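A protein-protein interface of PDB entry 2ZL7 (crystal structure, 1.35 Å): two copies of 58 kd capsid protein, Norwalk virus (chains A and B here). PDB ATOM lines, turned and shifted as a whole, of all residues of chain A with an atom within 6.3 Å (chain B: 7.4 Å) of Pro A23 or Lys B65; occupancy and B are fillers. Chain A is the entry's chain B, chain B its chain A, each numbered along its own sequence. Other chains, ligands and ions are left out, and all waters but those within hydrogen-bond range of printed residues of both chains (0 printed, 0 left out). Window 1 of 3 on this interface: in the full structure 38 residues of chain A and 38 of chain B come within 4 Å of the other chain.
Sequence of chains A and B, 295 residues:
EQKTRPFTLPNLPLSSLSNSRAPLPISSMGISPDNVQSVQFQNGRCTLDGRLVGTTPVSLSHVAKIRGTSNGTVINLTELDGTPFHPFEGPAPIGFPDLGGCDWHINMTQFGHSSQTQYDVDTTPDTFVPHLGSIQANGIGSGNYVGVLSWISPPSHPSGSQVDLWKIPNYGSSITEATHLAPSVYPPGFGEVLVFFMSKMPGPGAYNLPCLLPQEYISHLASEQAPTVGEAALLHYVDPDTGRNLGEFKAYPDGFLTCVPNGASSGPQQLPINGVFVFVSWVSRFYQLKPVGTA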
ATOM      1  N   SER A  18      14.500  -0.158 -11.820  1.00  0.00           N
ATOM      2  CA  SER A  18      14.712  -0.804 -10.530  1.00  0.00           C
ATOM      3  C   SER A  18      14.882   0.180  -9.413  1.00  0.00           C
ATOM      4  O   SER A  18      15.416   1.276  -9.597  1.00  0.00           O
ATOM      5  CB  SER A  18      15.996  -1.628 -10.536  1.00  0.00           C
ATOM      6  OG  SER A  18      16.138  -2.384  -9.329  1.00  0.00           O
ATOM      7  N   ASN A  19      14.488  -0.259  -8.216  1.00  0.00           N
ATOM      8  CA  ASN A  19      14.910   0.370  -6.986  1.00  0.00           C
ATOM      9  C   ASN A  19      16.448   0.354  -6.920  1.00  0.00           C
ATOM     10  O   ASN A  19      17.085  -0.518  -7.498  1.00  0.00           O
ATOM     11  CB  ASN A  19      14.337  -0.391  -5.772  1.00  0.00           C
ATOM     12  CG  ASN A  19      14.106   0.483  -4.573  1.00  0.00           C
ATOM     13  OD1 ASN A  19      15.034   0.817  -3.810  1.00  0.00           O
ATOM     14  ND2 ASN A  19      12.846   0.888  -4.397  1.00  0.00           N
ATOM     15  N   SER A  20      17.013   1.324  -6.204  1.00  0.00           N
ATOM     16  CA  SER A  20      18.446   1.377  -5.974  1.00  0.00           C
ATOM     17  C   SER A  20      18.840   0.921  -4.576  1.00  0.00           C
ATOM     18  O   SER A  20      20.030   0.900  -4.273  1.00  0.00           O
ATOM     19  CB  SER A  20      18.948   2.790  -6.259  1.00  0.00           C
ATOM     20  OG  SER A  20      18.190   3.735  -5.516  1.00  0.00           O
ATOM     21  N   ARG A  21      17.878   0.514  -3.727  1.00  0.00           N
ATOM     22  CA  ARG A  21      18.207  -0.035  -2.406  1.00  0.00           C
ATOM     23  C   ARG A  21      17.991  -1.547  -2.328  1.00  0.00           C
ATOM     24  O   ARG A  21      18.378  -2.173  -1.336  1.00  0.00           O
ATOM     25  CB  ARG A  21      17.429   0.700  -1.311  1.00  0.00           C
ATOM     26  CG  ARG A  21      17.872   2.130  -1.155  1.00  0.00           C
ATOM     27  CD  ARG A  21      16.984   2.918  -0.200  1.00  0.00           C
ATOM     28  NE  ARG A  21      17.234   2.517   1.188  1.00  0.00           N
ATOM     29  CZ  ARG A  21      16.404   2.731   2.206  1.00  0.00           C
ATOM     30  NH1 ARG A  21      15.198   3.218   2.000  1.00  0.00           N
ATOM     31  NH2 ARG A  21      16.764   2.390   3.430  1.00  0.00           N
ATOM     32  N   ALA A  22      17.361  -2.139  -3.339  1.00  0.00           N
ATOM     33  CA  ALA A  22      17.219  -3.585  -3.444  1.00  0.00           C
ATOM     34  C   ALA A  22      16.884  -3.859  -4.887  1.00  0.00           C
ATOM     35  O   ALA A  22      16.423  -2.965  -5.591  1.00  0.00           O
ATOM     36  CB  ALA A  22      16.110  -4.115  -2.516  1.00  0.00           C
ATOM     37  N   PRO A  23      17.158  -5.080  -5.349  1.00  0.00           N
ATOM     38  CA  PRO A  23      16.925  -5.405  -6.766  1.00  0.00           C
ATOM     39  C   PRO A  23      15.458  -5.705  -7.096  1.00  0.00           C
ATOM     40  O   PRO A  23      15.088  -6.839  -7.425  1.00  0.00           O
ATOM     41  CB  PRO A  23      17.826  -6.631  -6.988  1.00  0.00           C
ATOM     42  CG  PRO A  23      17.862  -7.300  -5.676  1.00  0.00           C
ATOM     43  CD  PRO A  23      17.867  -6.168  -4.651  1.00  0.00           C
ATOM     44  N   LEU A  24      14.630  -4.668  -7.030  1.00  0.00           N
ATOM     45  CA  LEU A  24      13.170  -4.791  -7.113  1.00  0.00           C
ATOM     46  C   LEU A  24      12.630  -3.813  -8.130  1.00  0.00           C
ATOM     47  O   LEU A  24      13.052  -2.664  -8.172  1.00  0.00           O
ATOM     48  CB  LEU A  24      12.542  -4.454  -5.768  1.00  0.00           C
ATOM     49  CG  LEU A  24      12.920  -5.328  -4.580  1.00  0.00           C
ATOM     50  CD1 LEU A  24      12.377  -4.706  -3.299  1.00  0.00           C
ATOM     51  CD2 LEU A  24      12.425  -6.759  -4.739  1.00  0.00           C
ATOM     52  N   PRO A  25      11.657  -4.231  -8.951  1.00  0.00           N
ATOM     53  CA  PRO A  25      10.997  -3.300  -9.865  1.00  0.00           C
ATOM     54  C   PRO A  25      10.372  -2.108  -9.146  1.00  0.00           C
ATOM     55  O   PRO A  25       9.889  -2.241  -8.022  1.00  0.00           O
ATOM     56  CB  PRO A  25       9.897  -4.169 -10.488  1.00  0.00           C
ATOM     57  CG  PRO A  25      10.414  -5.494 -10.438  1.00  0.00           C
ATOM     58  CD  PRO A  25      11.098  -5.580  -9.098  1.00  0.00           C
ATOM     59  N   LEU A  60      23.089  -2.694 -10.471  1.00  0.00           N
ATOM     60  CA  LEU A  60      22.182  -3.418  -9.595  1.00  0.00           C
ATOM     61  C   LEU A  60      22.731  -4.776  -9.177  1.00  0.00           C
ATOM     62  O   LEU A  60      22.312  -5.314  -8.149  1.00  0.00           O
ATOM     63  CB  LEU A  60      20.818  -3.590 -10.279  1.00  0.00           C
ATOM     64  CG  LEU A  60      19.673  -3.911  -9.319  1.00  0.00           C
ATOM     65  CD1 LEU A  60      19.234  -2.712  -8.489  1.00  0.00           C
ATOM     66  CD2 LEU A  60      18.509  -4.510 -10.117  1.00  0.00           C
ATOM     67  N   VAL A  63      23.776  -4.352  -5.657  1.00  0.00           N
ATOM     68  CA  VAL A  63      22.890  -3.705  -4.709  1.00  0.00           C
ATOM     69  C   VAL A  63      22.284  -4.669  -3.693  1.00  0.00           C
ATOM     70  O   VAL A  63      21.698  -5.696  -4.035  1.00  0.00           O
ATOM     71  CB  VAL A  63      21.764  -2.961  -5.454  1.00  0.00           C
ATOM     72  CG1 VAL A  63      20.653  -2.506  -4.488  1.00  0.00           C
ATOM     73  CG2 VAL A  63      22.370  -1.765  -6.181  1.00  0.00           C
ATOM     74  N   ALA A  64      22.437  -4.308  -2.428  1.00  0.00           N
ATOM     75  CA  ALA A  64      21.907  -5.051  -1.282  1.00  0.00           C
ATOM     76  C   ALA A  64      22.535  -6.437  -1.206  1.00  0.00           C
ATOM     77  O   ALA A  64      21.856  -7.457  -0.994  1.00  0.00           O
ATOM     78  CB  ALA A  64      20.351  -5.123  -1.321  1.00  0.00           C
ATOM     79  N   VAL A 148      22.583 -12.047  -0.951  1.00  0.00           N
ATOM     80  CA  VAL A 148      21.703 -11.001  -1.464  1.00  0.00           C
ATOM     81  C   VAL A 148      20.480 -10.890  -0.571  1.00  0.00           C
ATOM     82  O   VAL A 148      19.920 -11.913  -0.138  1.00  0.00           O
ATOM     83  CB  VAL A 148      21.325 -11.231  -2.945  1.00  0.00           C
ATOM     84  CG1 VAL A 148      20.561 -12.539  -3.149  1.00  0.00           C
ATOM     85  CG2 VAL A 148      20.523 -10.037  -3.492  1.00  0.00           C
ATOM     86  N   LEU A 149      20.058  -9.664  -0.291  1.00  0.00           N
ATOM     87  CA  LEU A 149      18.829  -9.456   0.474  1.00  0.00           C
ATOM     88  C   LEU A 149      17.655 -10.109  -0.243  1.00  0.00           C
ATOM     89  O   LEU A 149      17.441  -9.887  -1.449  1.00  0.00           O
ATOM     90  CB  LEU A 149      18.577  -7.967   0.626  1.00  0.00           C
ATOM     91  CG  LEU A 149      17.401  -7.540   1.502  1.00  0.00           C
ATOM     92  CD1 LEU A 149      17.531  -8.081   2.901  1.00  0.00           C
ATOM     93  CD2 LEU A 149      17.292  -6.031   1.534  1.00  0.00           C
ATOM     94  N   LEU A 209       9.541  -0.026  -0.249  1.00  0.00           N
ATOM     95  CA  LEU A 209      10.923   0.440  -0.078  1.00  0.00           C
ATOM     96  C   LEU A 209      11.148   1.684  -0.907  1.00  0.00           C
ATOM     97  O   LEU A 209      11.031   1.621  -2.141  1.00  0.00           O
ATOM     98  CB  LEU A 209      11.863  -0.650  -0.578  1.00  0.00           C
ATOM     99  CG  LEU A 209      13.360  -0.326  -0.604  1.00  0.00           C
ATOM    100  CD1 LEU A 209      13.915  -0.021   0.774  1.00  0.00           C
ATOM    101  CD2 LEU A 209      14.100  -1.484  -1.248  1.00  0.00           C
ATOM    102  N   ARG B  21      22.090 -12.294 -18.169  1.00  0.00           N
ATOM    103  CA  ARG B  21      21.355 -13.557 -18.019  1.00  0.00           C
ATOM    104  C   ARG B  21      21.154 -13.973 -16.569  1.00  0.00           C
ATOM    105  O   ARG B  21      20.418 -14.892 -16.291  1.00  0.00           O
ATOM    106  CB  ARG B  21      22.032 -14.675 -18.815  1.00  0.00           C
ATOM    107  CG  ARG B  21      21.950 -14.444 -20.308  1.00  0.00           C
ATOM    108  CD  ARG B  21      22.748 -15.466 -21.080  1.00  0.00           C
ATOM    109  NE  ARG B  21      22.129 -16.796 -21.072  1.00  0.00           N
ATOM    110  CZ  ARG B  21      22.770 -17.931 -21.314  1.00  0.00           C
ATOM    111  NH1 ARG B  21      24.073 -17.951 -21.466  1.00  0.00           N
ATOM    112  NH2 ARG B  21      22.099 -19.071 -21.364  1.00  0.00           N
ATOM    113  N   PRO B  23      21.662 -11.860 -12.329  1.00  0.00           N
ATOM    114  CA  PRO B  23      22.115 -10.641 -11.658  1.00  0.00           C
ATOM    115  C   PRO B  23      23.489 -10.757 -10.996  1.00  0.00           C
ATOM    116  O   PRO B  23      23.622 -10.684  -9.769  1.00  0.00           O
ATOM    117  CB  PRO B  23      20.990 -10.385 -10.657  1.00  0.00           C
ATOM    118  CG  PRO B  23      20.512 -11.769 -10.304  1.00  0.00           C
ATOM    119  CD  PRO B  23      20.576 -12.529 -11.591  1.00  0.00           C
ATOM    120  N   ASN B  43      17.669 -13.884 -23.070  1.00  0.00           N
ATOM    121  CA  ASN B  43      17.951 -12.679 -22.303  1.00  0.00           C
ATOM    122  C   ASN B  43      19.255 -12.057 -22.771  1.00  0.00           C
ATOM    123  O   ASN B  43      20.080 -12.717 -23.432  1.00  0.00           O
ATOM    124  CB  ASN B  43      17.967 -12.967 -20.810  1.00  0.00           C
ATOM    125  CG  ASN B  43      16.581 -13.232 -20.260  1.00  0.00           C
ATOM    126  OD1 ASN B  43      15.595 -12.647 -20.724  1.00  0.00           O
ATOM    127  ND2 ASN B  43      16.483 -14.107 -19.271  1.00  0.00           N
ATOM    128  N   SER B  59      15.627  -3.774 -17.268  1.00  0.00           N
ATOM    129  CA  SER B  59      16.260  -3.704 -15.956  1.00  0.00           C
ATOM    130  C   SER B  59      16.706  -5.047 -15.451  1.00  0.00           C
ATOM    131  O   SER B  59      15.986  -6.035 -15.551  1.00  0.00           O
ATOM    132  CB  SER B  59      15.279  -3.110 -14.930  1.00  0.00           C
ATOM    133  OG  SER B  59      15.801  -3.126 -13.606  1.00  0.00           O
ATOM    134  N   LEU B  60      17.852  -5.055 -14.788  1.00  0.00           N
ATOM    135  CA  LEU B  60      18.327  -6.235 -14.089  1.00  0.00           C
ATOM    136  C   LEU B  60      17.365  -6.720 -13.008  1.00  0.00           C
ATOM    137  O   LEU B  60      17.398  -7.899 -12.653  1.00  0.00           O
ATOM    138  CB  LEU B  60      19.697  -5.983 -13.469  1.00  0.00           C
ATOM    139  CG  LEU B  60      20.468  -7.256 -13.124  1.00  0.00           C
ATOM    140  CD1 LEU B  60      21.043  -7.960 -14.369  1.00  0.00           C
ATOM    141  CD2 LEU B  60      21.576  -6.888 -12.154  1.00  0.00           C
ATOM    142  N   SER B  61      16.500  -5.845 -12.493  1.00  0.00           N
ATOM    143  CA  SER B  61      15.522  -6.248 -11.493  1.00  0.00           C
ATOM    144  C   SER B  61      14.511  -7.247 -12.027  1.00  0.00           C
ATOM    145  O   SER B  61      13.775  -7.832 -11.246  1.00  0.00           O
ATOM    146  CB  SER B  61      14.827  -5.021 -10.901  1.00  0.00           C
ATOM    147  OG  SER B  61      14.051  -4.334 -11.870  1.00  0.00           O
ATOM    148  N   HIS B  62      14.478  -7.462 -13.333  1.00  0.00           N
ATOM    149  CA  HIS B  62      13.611  -8.477 -13.935  1.00  0.00           C
ATOM    150  C   HIS B  62      14.382  -9.699 -14.449  1.00  0.00           C
ATOM    151  O   HIS B  62      13.776 -10.635 -14.922  1.00  0.00           O
ATOM    152  CB  HIS B  62      12.884  -7.894 -15.143  1.00  0.00           C
ATOM    153  CG  HIS B  62      11.890  -6.818 -14.855  1.00  0.00           C
ATOM    154  ND1 HIS B  62      12.124  -5.672 -14.121  1.00  0.00           N
ATOM    155  CD2 HIS B  62      10.644  -6.680 -15.367  1.00  0.00           C
ATOM    156  CE1 HIS B  62      11.033  -4.909 -14.149  1.00  0.00           C
ATOM    157  NE2 HIS B  62      10.127  -5.505 -14.896  1.00  0.00           N
ATOM    158  N   VAL B  63      15.714  -9.697 -14.386  1.00  0.00           N
ATOM    159  CA  VAL B  63      16.524 -10.745 -15.022  1.00  0.00           C
ATOM    160  C   VAL B  63      16.608 -12.034 -14.205  1.00  0.00           C
ATOM    161  O   VAL B  63      16.970 -12.024 -13.031  1.00  0.00           O
ATOM    162  CB  VAL B  63      17.949 -10.211 -15.335  1.00  0.00           C
ATOM    163  CG1 VAL B  63      18.908 -11.354 -15.686  1.00  0.00           C
ATOM    164  CG2 VAL B  63      17.884  -9.212 -16.481  1.00  0.00           C
ATOM    165  N   ALA B  64      16.295 -13.141 -14.866  1.00  0.00           N
ATOM    166  CA  ALA B  64      16.317 -14.477 -14.284  1.00  0.00           C
ATOM    167  C   ALA B  64      15.371 -14.587 -13.104  1.00  0.00           C
ATOM    168  O   ALA B  64      15.695 -15.157 -12.059  1.00  0.00           O
ATOM    169  CB  ALA B  64      17.733 -14.894 -13.917  1.00  0.00           C
ATOM    170  N   LYS B  65      14.169 -14.069 -13.319  1.00  0.00           N
ATOM    171  CA  LYS B  65      13.114 -14.122 -12.330  1.00  0.00           C
ATOM    172  C   LYS B  65      11.863 -14.765 -12.889  1.00  0.00           C
ATOM    173  O   LYS B  65      11.661 -14.813 -14.108  1.00  0.00           O
ATOM    174  CB  LYS B  65      12.793 -12.732 -11.812  1.00  0.00           C
ATOM    175  CG  LYS B  65      13.929 -12.209 -10.952  1.00  0.00           C
ATOM    176  CD  LYS B  65      13.687 -10.822 -10.551  1.00  0.00           C
ATOM    177  CE  LYS B  65      12.958 -10.679  -9.312  1.00  0.00           C
ATOM    178  NZ  LYS B  65      13.389  -9.314  -8.808  1.00  0.00           N
ATOM    179  N   ILE B  66      11.060 -15.298 -11.972  1.00  0.00           N
ATOM    180  CA  ILE B  66       9.748 -15.870 -12.306  1.00  0.00           C
ATOM    181  C   ILE B  66       8.705 -15.301 -11.369  1.00  0.00           C
ATOM    182  O   ILE B  66       9.007 -14.855 -10.283  1.00  0.00           O
ATOM    183  CB  ILE B  66       9.747 -17.409 -12.245  1.00  0.00           C
ATOM    184  CG1 ILE B  66       9.859 -17.933 -10.817  1.00  0.00           C
ATOM    185  CG2 ILE B  66      10.899 -17.969 -13.083  1.00  0.00           C
ATOM    186  CD1 ILE B  66       9.669 -19.429 -10.713  1.00  0.00           C
ATOM    187  N   ARG B  67       7.460 -15.306 -11.820  1.00  0.00           N
ATOM    188  CA  ARG B  67       6.347 -15.010 -10.965  1.00  0.00           C
ATOM    189  C   ARG B  67       5.201 -15.919 -11.322  1.00  0.00           C
ATOM    190  O   ARG B  67       4.898 -16.124 -12.490  1.00  0.00           O
ATOM    191  CB  ARG B  67       5.908 -13.577 -11.118  1.00  0.00           C
ATOM    192  CG  ARG B  67       4.745 -13.311 -10.204  1.00  0.00           C
ATOM    193  CD  ARG B  67       4.772 -12.036  -9.603  1.00  0.00           C
ATOM    194  NE  ARG B  67       3.879 -11.970  -8.448  1.00  0.00           N
ATOM    195  CZ  ARG B  67       3.339 -10.829  -8.072  1.00  0.00           C
ATOM    196  NH1 ARG B  67       3.617  -9.717  -8.734  1.00  0.00           N
ATOM    197  NH2 ARG B  67       2.511 -10.795  -7.038  1.00  0.00           N
ATOM    198  N   LEU B  77       2.358 -19.231 -14.515  1.00  0.00           N
ATOM    199  CA  LEU B  77       3.213 -18.053 -14.600  1.00  0.00           C
ATOM    200  C   LEU B  77       2.453 -16.829 -15.051  1.00  0.00           C
ATOM    201  O   LEU B  77       1.505 -16.929 -15.845  1.00  0.00           O
ATOM    202  CB  LEU B  77       4.333 -18.324 -15.601  1.00  0.00           C
ATOM    203  CG  LEU B  77       5.282 -19.469 -15.265  1.00  0.00           C
ATOM    204  CD1 LEU B  77       6.178 -19.734 -16.472  1.00  0.00           C
ATOM    205  CD2 LEU B  77       6.103 -19.143 -14.022  1.00  0.00           C
ATOM    206  N   THR B  78       2.905 -15.677 -14.575  1.00  0.00           N
ATOM    207  CA  THR B  78       2.497 -14.375 -15.063  1.00  0.00           C
ATOM    208  C   THR B  78       3.762 -13.571 -15.380  1.00  0.00           C
ATOM    209  O   THR B  78       4.877 -14.043 -15.155  1.00  0.00           O
ATOM    210  CB  THR B  78       1.687 -13.608 -13.989  1.00  0.00           C
ATOM    211  OG1 THR B  78       2.509 -13.358 -12.837  1.00  0.00           O
ATOM    212  CG2 THR B  78       0.432 -14.385 -13.555  1.00  0.00           C
ATOM    213  N   LEU B  80       6.245 -10.487 -14.235  1.00  0.00           N
ATOM    214  CA  LEU B  80       6.778 -10.195 -12.908  1.00  0.00           C
ATOM    215  C   LEU B  80       5.850  -9.306 -12.098  1.00  0.00           C
ATOM    216  O   LEU B  80       5.729  -9.485 -10.884  1.00  0.00           O
ATOM    217  CB  LEU B  80       8.177  -9.568 -13.014  1.00  0.00           C
ATOM    218  CG  LEU B  80       8.950  -9.314 -11.735  1.00  0.00           C
ATOM    219  CD1 LEU B  80       9.194 -10.648 -11.040  1.00  0.00           C
ATOM    220  CD2 LEU B  80      10.278  -8.569 -12.031  1.00  0.00           C
ATOM    221  N   PRO B  93       7.579 -15.616 -19.988  1.00  0.00           N
ATOM    222  CA  PRO B  93       7.436 -14.226 -19.580  1.00  0.00           C
ATOM    223  C   PRO B  93       8.768 -13.464 -19.625  1.00  0.00           C
ATOM    224  O   PRO B  93       9.867 -14.060 -19.504  1.00  0.00           O
ATOM    225  CB  PRO B  93       6.897 -14.341 -18.146  1.00  0.00           C
ATOM    226  CG  PRO B  93       6.232 -15.697 -18.116  1.00  0.00           C
ATOM    227  CD  PRO B  93       7.105 -16.548 -18.952  1.00  0.00           C
ATOM    228  N   ILE B  94       8.677 -12.144 -19.731  1.00  0.00           N
ATOM    229  CA  ILE B  94       9.859 -11.291 -19.716  1.00  0.00           C
ATOM    230  C   ILE B  94      10.720 -11.605 -18.479  1.00  0.00           C
ATOM    231  O   ILE B  94      10.214 -11.734 -17.372  1.00  0.00           O
ATOM    232  CB  ILE B  94       9.467  -9.797 -19.758  1.00  0.00           C
ATOM    233  CG1 ILE B  94       8.778  -9.459 -21.082  1.00  0.00           C
ATOM    234  CG2 ILE B  94      10.681  -8.916 -19.503  1.00  0.00           C
ATOM    235  CD1 ILE B  94       9.607  -9.691 -22.311  1.00  0.00           C
ATOM    236  N   GLY B  95      12.021 -11.762 -18.700  1.00  0.00           N
ATOM    237  CA  GLY B  95      12.981 -11.994 -17.630  1.00  0.00           C
ATOM    238  C   GLY B  95      13.152 -13.435 -17.238  1.00  0.00           C
ATOM    239  O   GLY B  95      14.054 -13.745 -16.470  1.00  0.00           O
ATOM    240  N   PHE B  96      12.317 -14.330 -17.741  1.00  0.00           N
ATOM    241  CA  PHE B  96      12.370 -15.724 -17.327  1.00  0.00           C
ATOM    242  C   PHE B  96      13.783 -16.264 -17.579  1.00  0.00           C
ATOM    243  O   PHE B  96      14.388 -15.937 -18.588  1.00  0.00           O
ATOM    244  CB  PHE B  96      11.346 -16.517 -18.130  1.00  0.00           C
ATOM    245  CG  PHE B  96      11.072 -17.901 -17.611  1.00  0.00           C
ATOM    246  CD1 PHE B  96      10.121 -18.124 -16.617  1.00  0.00           C
ATOM    247  CD2 PHE B  96      11.742 -18.980 -18.142  1.00  0.00           C
ATOM    248  CE1 PHE B  96       9.869 -19.418 -16.174  1.00  0.00           C
ATOM    249  CE2 PHE B  96      11.474 -20.265 -17.694  1.00  0.00           C
ATOM    250  CZ  PHE B  96      10.552 -20.466 -16.710  1.00  0.00           C
ATOM    251  N   PRO B  97      14.344 -17.091 -16.672  1.00  0.00           N
ATOM    252  CA  PRO B  97      15.698 -17.551 -16.936  1.00  0.00           C
ATOM    253  C   PRO B  97      15.879 -18.273 -18.256  1.00  0.00           C
ATOM    254  O   PRO B  97      14.975 -19.004 -18.696  1.00  0.00           O
ATOM    255  CB  PRO B  97      15.998 -18.478 -15.749  1.00  0.00           C
ATOM    256  CG  PRO B  97      15.050 -18.055 -14.655  1.00  0.00           C
ATOM    257  CD  PRO B  97      13.816 -17.590 -15.395  1.00  0.00           C
ATOM    258  N   ILE B 106      15.964 -21.812  -7.618  1.00  0.00           N
ATOM    259  CA  ILE B 106      15.364 -20.500  -7.609  1.00  0.00           C
ATOM    260  C   ILE B 106      14.893 -20.175  -6.208  1.00  0.00           C
ATOM    261  O   ILE B 106      14.258 -21.008  -5.556  1.00  0.00           O
ATOM    262  CB  ILE B 106      14.185 -20.454  -8.611  1.00  0.00           C
ATOM    263  CG1 ILE B 106      14.723 -20.476 -10.044  1.00  0.00           C
ATOM    264  CG2 ILE B 106      13.307 -19.201  -8.403  1.00  0.00           C
ATOM    265  CD1 ILE B 106      13.660 -20.571 -11.088  1.00  0.00           C
ATOM    266  N   VAL B 146       7.282 -14.784  -6.088  1.00  0.00           N
ATOM    267  CA  VAL B 146       8.323 -14.267  -6.996  1.00  0.00           C
ATOM    268  C   VAL B 146       9.579 -15.071  -6.706  1.00  0.00           C
ATOM    269  O   VAL B 146       9.906 -15.340  -5.539  1.00  0.00           O
ATOM    270  CB  VAL B 146       8.607 -12.780  -6.795  1.00  0.00           C
ATOM    271  CG1 VAL B 146       9.060 -12.484  -5.398  1.00  0.00           C
ATOM    272  CG2 VAL B 146       9.669 -12.279  -7.796  1.00  0.00           C
ATOM    273  N   GLY B 147      10.262 -15.493  -7.763  1.00  0.00           N
ATOM    274  CA  GLY B 147      11.488 -16.259  -7.629  1.00  0.00           C
ATOM    275  C   GLY B 147      12.622 -15.603  -8.392  1.00  0.00           C
ATOM    276  O   GLY B 147      12.400 -15.004  -9.453  1.00  0.00           O
ATOM    277  N   VAL B 148      13.833 -15.764  -7.876  1.00  0.00           N
ATOM    278  CA  VAL B 148      15.031 -15.315  -8.580  1.00  0.00           C
ATOM    279  C   VAL B 148      16.034 -16.459  -8.593  1.00  0.00           C
ATOM    280  O   VAL B 148      16.222 -17.163  -7.602  1.00  0.00           O
ATOM    281  CB  VAL B 148      15.642 -14.057  -7.940  1.00  0.00           C
ATOM    282  CG1 VAL B 148      16.060 -14.310  -6.498  1.00  0.00           C
ATOM    283  CG2 VAL B 148      16.783 -13.501  -8.793  1.00  0.00           C
ATOM    284  N   LEU B 149      16.682 -16.652  -9.728  1.00  0.00           N
ATOM    285  CA  LEU B 149      17.691 -17.675  -9.843  1.00  0.00           C
ATOM    286  C   LEU B 149      18.797 -17.425  -8.821  1.00  0.00           C
ATOM    287  O   LEU B 149      19.312 -16.309  -8.717  1.00  0.00           O
ATOM    288  CB  LEU B 149      18.282 -17.657 -11.238  1.00  0.00           C
ATOM    289  CG  LEU B 149      19.333 -18.726 -11.554  1.00  0.00           C
ATOM    290  CD1 LEU B 149      18.812 -20.151 -11.400  1.00  0.00           C
ATOM    291  CD2 LEU B 149      19.897 -18.496 -12.965  1.00  0.00           C
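The side-chain amino group of Lys B65 lies within hydrogen-bond range of the backbone carbonyl oxygen of Pro A23.
The side-chain hydroxyl (OG) of Ser B59 sits at hydrogen-bond distance from the side-chain hydroxyl (OG) of Ser B61 (2.7 Å).
The side-chain hydroxyl (OG) of Ser B61 lies within hydrogen-bond range of a ring nitrogen (ND1) of His B62 (3.3 Å).
The backbone carbonyl oxygen (O) of Ser B61 sits at hydrogen-bond distance from the side-chain amino group (NZ) of Lys B65.
NH1 of Arg B67 lies close to O of Leu B80 (3.0 Å).
The backbone carbonyl oxygen (O) of Leu A24 sits at hydrogen-bond distance from the side-chain hydroxyl (OG) of Ser A18 (3.3 Å).
N of Asn A19 sits at hydrogen-bond distance from O of Leu A24.
OG of Ser B59 touches CB of Ser A18, at 3.4 Å.
Ser B61 touches Ser A18 (CB to OG, 3.3 Å).
Ser B61 touches Pro A23.
Leu A24 touches Ser B61 (C to CB, 3.7 Å).
N of Pro A25 touches OG of Ser B61, at 3.8 Å.
His B62 touches Pro A25 (CE1 to CG, 3.8 Å).
CG of Pro A25 touches CD2 of Leu B80, at 3.5 Å.
CD2 of Leu A60 touches C of Leu B60, at 3.8 Å.
CD2 of Leu A60 touches N of Ser B61, 3.4 Å away.
Of chain B, only Ser B61 (3.9 Å) and Lys B65 (3.3 Å) come within 4 Å of Pro A23.
Printed residues of chain B within 4 Å of Pro A25: Ser B61, His B62 and Leu B80.
Of the printed residues of chain B, Leu A60 touches Leu B60 and Ser B61.
Of the printed residues of chain A, Lys B65 touches Pro A23 (3.3 Å).
Printed residues of chain A within 4 Å of Leu B80: Pro A25.
The nearest residue of chain A that does not touch Lys B65 is Pro A25 (4.4 Å).
The nearest printed residue of chain B that does not touch Ser A18 is Leu B60 (5.8 Å).
Of the 25 printed residues of chain B, 6 touch a printed residue of chain A.
Printed residues of chain A that touch a printed residue of chain B: Ser A18, Pro A23, Leu A24, Pro A25 and Leu A60.
Among the printed residues, 10 pairs touch across the chains.
Among the printed residues, no Asp or Glu carboxylate lies within 4 Å of a Lys or Arg side-chain nitrogen of the other chain.
Leu A60 touches its own counterpart, Leu B60.
7 positions are printed for both chains.
Of the 10 pairs that touch across the chains among the printed residues, 1 has its exchanged pair printed and touching as well.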
